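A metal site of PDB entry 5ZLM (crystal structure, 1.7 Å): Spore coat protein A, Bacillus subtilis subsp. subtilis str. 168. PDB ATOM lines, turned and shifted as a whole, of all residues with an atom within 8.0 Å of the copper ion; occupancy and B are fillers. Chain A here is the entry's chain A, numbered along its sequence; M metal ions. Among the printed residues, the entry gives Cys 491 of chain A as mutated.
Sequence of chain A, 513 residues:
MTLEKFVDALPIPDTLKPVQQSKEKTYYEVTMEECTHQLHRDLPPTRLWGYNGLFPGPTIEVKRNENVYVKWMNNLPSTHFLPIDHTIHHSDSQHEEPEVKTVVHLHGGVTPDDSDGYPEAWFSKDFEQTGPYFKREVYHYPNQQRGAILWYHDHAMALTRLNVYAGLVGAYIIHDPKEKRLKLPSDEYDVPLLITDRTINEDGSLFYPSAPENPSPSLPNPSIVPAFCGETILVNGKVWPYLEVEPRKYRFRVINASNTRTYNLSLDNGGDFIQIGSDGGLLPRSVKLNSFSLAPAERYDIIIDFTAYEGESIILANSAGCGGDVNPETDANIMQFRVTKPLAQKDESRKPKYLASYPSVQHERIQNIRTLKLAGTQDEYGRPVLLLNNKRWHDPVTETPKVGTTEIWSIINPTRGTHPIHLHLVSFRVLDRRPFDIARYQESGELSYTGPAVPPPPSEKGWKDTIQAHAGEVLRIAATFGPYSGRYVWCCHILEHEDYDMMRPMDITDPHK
N of Met 502 sits at hydrogen-bond distance from O of His 497 (2.9 Å).
The backbone NH (N) of Ile 494 lies close to the side-chain sulfur (SG) of Cys 492.
A ring nitrogen (NE2) of His 497 lies close to the backbone carbonyl oxygen of Pro 226, 3.1 Å away.
O of His 419 lies within hydrogen-bond range of N of Ala 469, at 2.9 Å.
N of Cys 492 sits at hydrogen-bond distance from O of Met 502, at 3.0 Å.
A ring nitrogen (NE2) of His 419 sits at hydrogen-bond distance from the side-chain hydroxyl of Thr 415 (3.1 Å).
A ring nitrogen (ND1) of His 419 lies close to the side-chain sulfur (SD) of Met 502, 3.6 Å away.
The backbone carbonyl oxygen of Leu 386 is in hydrogen-bond range of the backbone NH of Met 502.
Residues that only touch the copper ion: Ile 494 (3.97 Å) and Met 502 (3.1 Å).
Five residues have an atom within 4 Å of the copper ion: His 419, Cys 492, Ile 494, His 497 and Met 502.
The copper ion is bound by ND1 of His 419 (2.1 Å), ND1 of His 497 (2.1 Å) and SG of Cys 492 (2.2 Å).
The copper ion has three donor atoms within binding distance.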
ATOM      1  N   PRO A 226       7.684  24.816 -24.811  1.00  0.00           N
ATOM      2  CA  PRO A 226       8.898  25.272 -24.110  1.00  0.00           C
ATOM      3  C   PRO A 226      10.103  24.422 -24.318  1.00  0.00           C
ATOM      4  O   PRO A 226      11.164  24.795 -23.833  1.00  0.00           O
ATOM      5  CB  PRO A 226       8.485  25.240 -22.617  1.00  0.00           C
ATOM      6  CG  PRO A 226       7.422  24.240 -22.565  1.00  0.00           C
ATOM      7  CD  PRO A 226       6.692  24.253 -23.881  1.00  0.00           C
ATOM      8  N   LEU A 374      18.245  33.764 -14.112  1.00  0.00           N
ATOM      9  CA  LEU A 374      17.409  33.051 -15.092  1.00  0.00           C
ATOM     10  C   LEU A 374      16.054  32.683 -14.493  1.00  0.00           C
ATOM     11  O   LEU A 374      15.990  31.955 -13.515  1.00  0.00           O
ATOM     12  CB  LEU A 374      18.144  31.769 -15.509  1.00  0.00           C
ATOM     13  CG  LEU A 374      19.602  31.935 -15.945  1.00  0.00           C
ATOM     14  CD1 LEU A 374      20.164  30.597 -16.393  1.00  0.00           C
ATOM     15  CD2 LEU A 374      19.772  32.966 -17.028  1.00  0.00           C
ATOM     16  N   LEU A 386      10.167  32.587 -20.559  1.00  0.00           N
ATOM     17  CA  LEU A 386      11.461  32.496 -19.887  1.00  0.00           C
ATOM     18  C   LEU A 386      12.254  33.780 -20.127  1.00  0.00           C
ATOM     19  O   LEU A 386      12.312  34.244 -21.263  1.00  0.00           O
ATOM     20  CB  LEU A 386      12.278  31.301 -20.397  1.00  0.00           C
ATOM     21  CG  LEU A 386      11.816  30.024 -19.723  1.00  0.00           C
ATOM     22  CD1 LEU A 386      12.094  28.795 -20.542  1.00  0.00           C
ATOM     23  CD2 LEU A 386      12.483  29.905 -18.345  1.00  0.00           C
ATOM     24  N   LEU A 387      12.826  34.360 -19.065  1.00  0.00           N
ATOM     25  CA  LEU A 387      13.422  35.677 -19.151  1.00  0.00           C
ATOM     26  C   LEU A 387      14.822  35.702 -18.572  1.00  0.00           C
ATOM     27  O   LEU A 387      15.160  34.980 -17.594  1.00  0.00           O
ATOM     28  CB  LEU A 387      12.569  36.721 -18.423  1.00  0.00           C
ATOM     29  CG  LEU A 387      11.101  36.845 -18.749  1.00  0.00           C
ATOM     30  CD1 LEU A 387      10.445  37.896 -17.850  1.00  0.00           C
ATOM     31  CD2 LEU A 387      10.899  37.234 -20.186  1.00  0.00           C
ATOM     32  N   LEU A 388      15.647  36.559 -19.184  1.00  0.00           N
ATOM     33  CA  LEU A 388      16.949  36.851 -18.665  1.00  0.00           C
ATOM     34  C   LEU A 388      16.869  38.099 -17.751  1.00  0.00           C
ATOM     35  O   LEU A 388      16.593  39.221 -18.213  1.00  0.00           O
ATOM     36  CB  LEU A 388      17.926  37.141 -19.801  1.00  0.00           C
ATOM     37  CG  LEU A 388      18.173  35.949 -20.756  1.00  0.00           C
ATOM     38  CD1 LEU A 388      19.023  36.366 -21.922  1.00  0.00           C
ATOM     39  CD2 LEU A 388      18.793  34.766 -20.024  1.00  0.00           C
ATOM     40  N   ASN A 413      20.819  30.449 -11.531  1.00  0.00           N
ATOM     41  CA  ASN A 413      19.775  29.609 -12.090  1.00  0.00           C
ATOM     42  C   ASN A 413      18.949  28.891 -11.038  1.00  0.00           C
ATOM     43  O   ASN A 413      19.306  27.789 -10.615  1.00  0.00           O
ATOM     44  CB  ASN A 413      20.344  28.557 -13.045  1.00  0.00           C
ATOM     45  CG  ASN A 413      19.264  27.707 -13.678  1.00  0.00           C
ATOM     46  OD1 ASN A 413      18.059  27.923 -13.490  1.00  0.00           O
ATOM     47  ND2 ASN A 413      19.674  26.741 -14.485  1.00  0.00           N
ATOM     48  N   THR A 415      15.920  27.786 -11.678  1.00  0.00           N
ATOM     49  CA  THR A 415      14.931  26.977 -12.376  1.00  0.00           C
ATOM     50  C   THR A 415      15.284  25.478 -12.262  1.00  0.00           C
ATOM     51  O   THR A 415      16.334  25.104 -11.743  1.00  0.00           O
ATOM     52  CB  THR A 415      14.796  27.392 -13.861  1.00  0.00           C
ATOM     53  OG1 THR A 415      15.896  26.851 -14.621  1.00  0.00           O
ATOM     54  CG2 THR A 415      14.762  28.930 -14.018  1.00  0.00           C
ATOM     55  N   GLY A 417      15.944  23.258 -14.684  1.00  0.00           N
ATOM     56  CA  GLY A 417      16.818  22.639 -15.689  1.00  0.00           C
ATOM     57  C   GLY A 417      17.973  23.518 -16.086  1.00  0.00           C
ATOM     58  O   GLY A 417      18.081  24.648 -15.649  1.00  0.00           O
ATOM     59  N   THR A 418      18.873  22.945 -16.877  1.00  0.00           N
ATOM     60  CA  THR A 418      20.037  23.636 -17.365  1.00  0.00           C
ATOM     61  C   THR A 418      19.686  24.551 -18.540  1.00  0.00           C
ATOM     62  O   THR A 418      18.850  24.223 -19.384  1.00  0.00           O
ATOM     63  CB  THR A 418      21.114  22.622 -17.820  1.00  0.00           C
ATOM     64  OG1 THR A 418      21.499  21.782 -16.726  1.00  0.00           O
ATOM     65  CG2 THR A 418      22.329  23.262 -18.422  1.00  0.00           C
ATOM     66  N   HIS A 419      20.319  25.726 -18.587  1.00  0.00           N
ATOM     67  CA  HIS A 419      20.204  26.651 -19.744  1.00  0.00           C
ATOM     68  C   HIS A 419      21.599  26.825 -20.305  1.00  0.00           C
ATOM     69  O   HIS A 419      22.544  27.148 -19.594  1.00  0.00           O
ATOM     70  CB  HIS A 419      19.635  27.995 -19.317  1.00  0.00           C
ATOM     71  CG  HIS A 419      18.275  27.909 -18.727  1.00  0.00           C
ATOM     72  ND1 HIS A 419      17.154  27.903 -19.505  1.00  0.00           N
ATOM     73  CD2 HIS A 419      17.841  27.782 -17.439  1.00  0.00           C
ATOM     74  CE1 HIS A 419      16.085  27.821 -18.751  1.00  0.00           C
ATOM     75  NE2 HIS A 419      16.463  27.726 -17.491  1.00  0.00           N
ATOM     76  N   PRO A 420      21.778  26.606 -21.639  1.00  0.00           N
ATOM     77  CA  PRO A 420      23.025  26.879 -22.315  1.00  0.00           C
ATOM     78  C   PRO A 420      23.119  28.361 -22.722  1.00  0.00           C
ATOM     79  O   PRO A 420      22.530  28.796 -23.706  1.00  0.00           O
ATOM     80  CB  PRO A 420      22.957  25.916 -23.532  1.00  0.00           C
ATOM     81  CG  PRO A 420      21.495  25.863 -23.859  1.00  0.00           C
ATOM     82  CD  PRO A 420      20.771  26.027 -22.561  1.00  0.00           C
ATOM     83  N   ILE A 421      23.794  29.143 -21.901  1.00  0.00           N
ATOM     84  CA  ILE A 421      23.870  30.593 -22.104  1.00  0.00           C
ATOM     85  C   ILE A 421      24.971  30.970 -23.102  1.00  0.00           C
ATOM     86  O   ILE A 421      26.112  30.504 -22.944  1.00  0.00           O
ATOM     87  CB  ILE A 421      24.095  31.295 -20.743  1.00  0.00           C
ATOM     88  CG1 ILE A 421      22.944  30.969 -19.807  1.00  0.00           C
ATOM     89  CG2 ILE A 421      24.301  32.780 -20.986  1.00  0.00           C
ATOM     90  CD1 ILE A 421      21.556  31.360 -20.299  1.00  0.00           C
ATOM     91  N   ALA A 469      24.575  26.513 -17.657  1.00  0.00           N
ATOM     92  CA  ALA A 469      24.225  27.007 -16.321  1.00  0.00           C
ATOM     93  C   ALA A 469      23.238  26.053 -15.745  1.00  0.00           C
ATOM     94  O   ALA A 469      22.052  26.085 -16.064  1.00  0.00           O
ATOM     95  CB  ALA A 469      23.667  28.427 -16.404  1.00  0.00           C
ATOM     96  N   CYS A 491      21.948  35.277 -24.831  1.00  0.00           N
ATOM     97  CA  CYS A 491      20.726  34.481 -24.953  1.00  0.00           C
ATOM     98  C   CYS A 491      20.879  33.095 -24.370  1.00  0.00           C
ATOM     99  O   CYS A 491      22.015  32.644 -24.080  1.00  0.00           O
ATOM    100  CB  CYS A 491      20.329  34.397 -26.415  1.00  0.00           C
ATOM    101  SG  CYS A 491      21.599  33.669 -27.492  1.00  0.00           S
ATOM    102  N   CYS A 492      19.765  32.439 -24.134  1.00  0.00           N
ATOM    103  CA  CYS A 492      19.748  31.019 -23.916  1.00  0.00           C
ATOM    104  C   CYS A 492      19.596  30.360 -25.277  1.00  0.00           C
ATOM    105  O   CYS A 492      18.743  30.761 -26.063  1.00  0.00           O
ATOM    106  CB  CYS A 492      18.619  30.591 -23.007  1.00  0.00           C
ATOM    107  SG  CYS A 492      18.453  28.807 -22.903  1.00  0.00           S
ATOM    108  N   HIS A 493      20.413  29.346 -25.520  1.00  0.00           N
ATOM    109  CA  HIS A 493      20.401  28.665 -26.808  1.00  0.00           C
ATOM    110  C   HIS A 493      19.490  27.449 -26.911  1.00  0.00           C
ATOM    111  O   HIS A 493      19.581  26.667 -27.911  1.00  0.00           O
ATOM    112  CB  HIS A 493      21.826  28.344 -27.275  1.00  0.00           C
ATOM    113  CG  HIS A 493      22.020  28.643 -28.715  1.00  0.00           C
ATOM    114  ND1 HIS A 493      21.585  27.788 -29.690  1.00  0.00           N
ATOM    115  CD2 HIS A 493      22.546  29.712 -29.353  1.00  0.00           C
ATOM    116  CE1 HIS A 493      21.844  28.297 -30.871  1.00  0.00           C
ATOM    117  NE2 HIS A 493      22.423  29.463 -30.700  1.00  0.00           N
ATOM    118  N   ILE A 494      18.593  27.254 -25.961  1.00  0.00           N
ATOM    119  CA  ILE A 494      17.446  26.386 -26.166  1.00  0.00           C
ATOM    120  C   ILE A 494      16.476  27.244 -26.962  1.00  0.00           C
ATOM    121  O   ILE A 494      15.934  28.237 -26.466  1.00  0.00           O
ATOM    122  CB  ILE A 494      16.808  25.851 -24.862  1.00  0.00           C
ATOM    123  CG1 ILE A 494      17.772  24.907 -24.152  1.00  0.00           C
ATOM    124  CG2 ILE A 494      15.467  25.131 -25.182  1.00  0.00           C
ATOM    125  CD1 ILE A 494      17.360  24.570 -22.738  1.00  0.00           C
ATOM    126  N   LEU A 495      16.303  26.927 -28.236  1.00  0.00           N
ATOM    127  CA  LEU A 495      15.635  27.843 -29.127  1.00  0.00           C
ATOM    128  C   LEU A 495      14.177  28.116 -28.718  1.00  0.00           C
ATOM    129  O   LEU A 495      13.694  29.219 -28.902  1.00  0.00           O
ATOM    130  CB  LEU A 495      15.760  27.372 -30.581  1.00  0.00           C
ATOM    131  CG  LEU A 495      17.218  27.149 -31.020  1.00  0.00           C
ATOM    132  CD1 LEU A 495      17.174  26.831 -32.523  1.00  0.00           C
ATOM    133  CD2 LEU A 495      18.086  28.387 -30.800  1.00  0.00           C
ATOM    134  N   GLU A 496      13.504  27.104 -28.188  1.00  0.00           N
ATOM    135  CA  GLU A 496      12.148  27.252 -27.672  1.00  0.00           C
ATOM    136  C   GLU A 496      12.087  28.284 -26.516  1.00  0.00           C
ATOM    137  O   GLU A 496      11.022  28.923 -26.316  1.00  0.00           O
ATOM    138  CB  GLU A 496      11.620  25.906 -27.231  1.00  0.00           C
ATOM    139  CG  GLU A 496      11.189  24.979 -28.369  1.00  0.00           C
ATOM    140  CD  GLU A 496      12.325  24.446 -29.241  1.00  0.00           C
ATOM    141  OE1 GLU A 496      13.482  24.341 -28.769  1.00  0.00           O
ATOM    142  OE2 GLU A 496      12.030  24.132 -30.442  1.00  0.00           O
ATOM    143  N   HIS A 497      13.196  28.419 -25.779  1.00  0.00           N
ATOM    144  CA  HIS A 497      13.337  29.442 -24.679  1.00  0.00           C
ATOM    145  C   HIS A 497      13.676  30.782 -25.301  1.00  0.00           C
ATOM    146  O   HIS A 497      13.045  31.818 -25.003  1.00  0.00           O
ATOM    147  CB  HIS A 497      14.420  29.088 -23.664  1.00  0.00           C
ATOM    148  CG  HIS A 497      14.176  27.824 -22.908  1.00  0.00           C
ATOM    149  ND1 HIS A 497      15.025  27.362 -21.935  1.00  0.00           N
ATOM    150  CD2 HIS A 497      13.160  26.939 -22.978  1.00  0.00           C
ATOM    151  CE1 HIS A 497      14.538  26.225 -21.436  1.00  0.00           C
ATOM    152  NE2 HIS A 497      13.398  25.959 -22.050  1.00  0.00           N
ATOM    153  N   GLU A 498      14.695  30.775 -26.143  1.00  0.00           N
ATOM    154  CA  GLU A 498      15.141  31.981 -26.833  1.00  0.00           C
ATOM    155  C   GLU A 498      14.001  32.789 -27.454  1.00  0.00           C
ATOM    156  O   GLU A 498      13.956  34.010 -27.346  1.00  0.00           O
ATOM    157  CB  GLU A 498      16.191  31.555 -27.904  1.00  0.00           C
ATOM    158  CG  GLU A 498      16.965  32.707 -28.478  1.00  0.00           C
ATOM    159  CD  GLU A 498      17.988  32.225 -29.503  1.00  0.00           C
ATOM    160  OE1 GLU A 498      18.849  31.400 -29.189  1.00  0.00           O
ATOM    161  OE2 GLU A 498      17.919  32.706 -30.620  1.00  0.00           O
ATOM    162  N   MET A 502      13.854  34.408 -23.933  1.00  0.00           N
ATOM    163  CA  MET A 502      15.085  34.321 -23.158  1.00  0.00           C
ATOM    164  C   MET A 502      16.318  34.792 -23.980  1.00  0.00           C
ATOM    165  O   MET A 502      17.234  34.032 -24.276  1.00  0.00           O
ATOM    166  CB  MET A 502      15.234  32.919 -22.612  1.00  0.00           C
ATOM    167  CG  MET A 502      16.114  32.781 -21.394  1.00  0.00           C
ATOM    168  SD  MET A 502      15.988  31.146 -20.705  1.00  0.00           S
ATOM    169  CE  MET A 502      17.086  31.242 -19.320  1.00  0.00           C
HETATM  170 CU    CU M   1      16.860  28.310 -21.506  1.00  0.00          CU
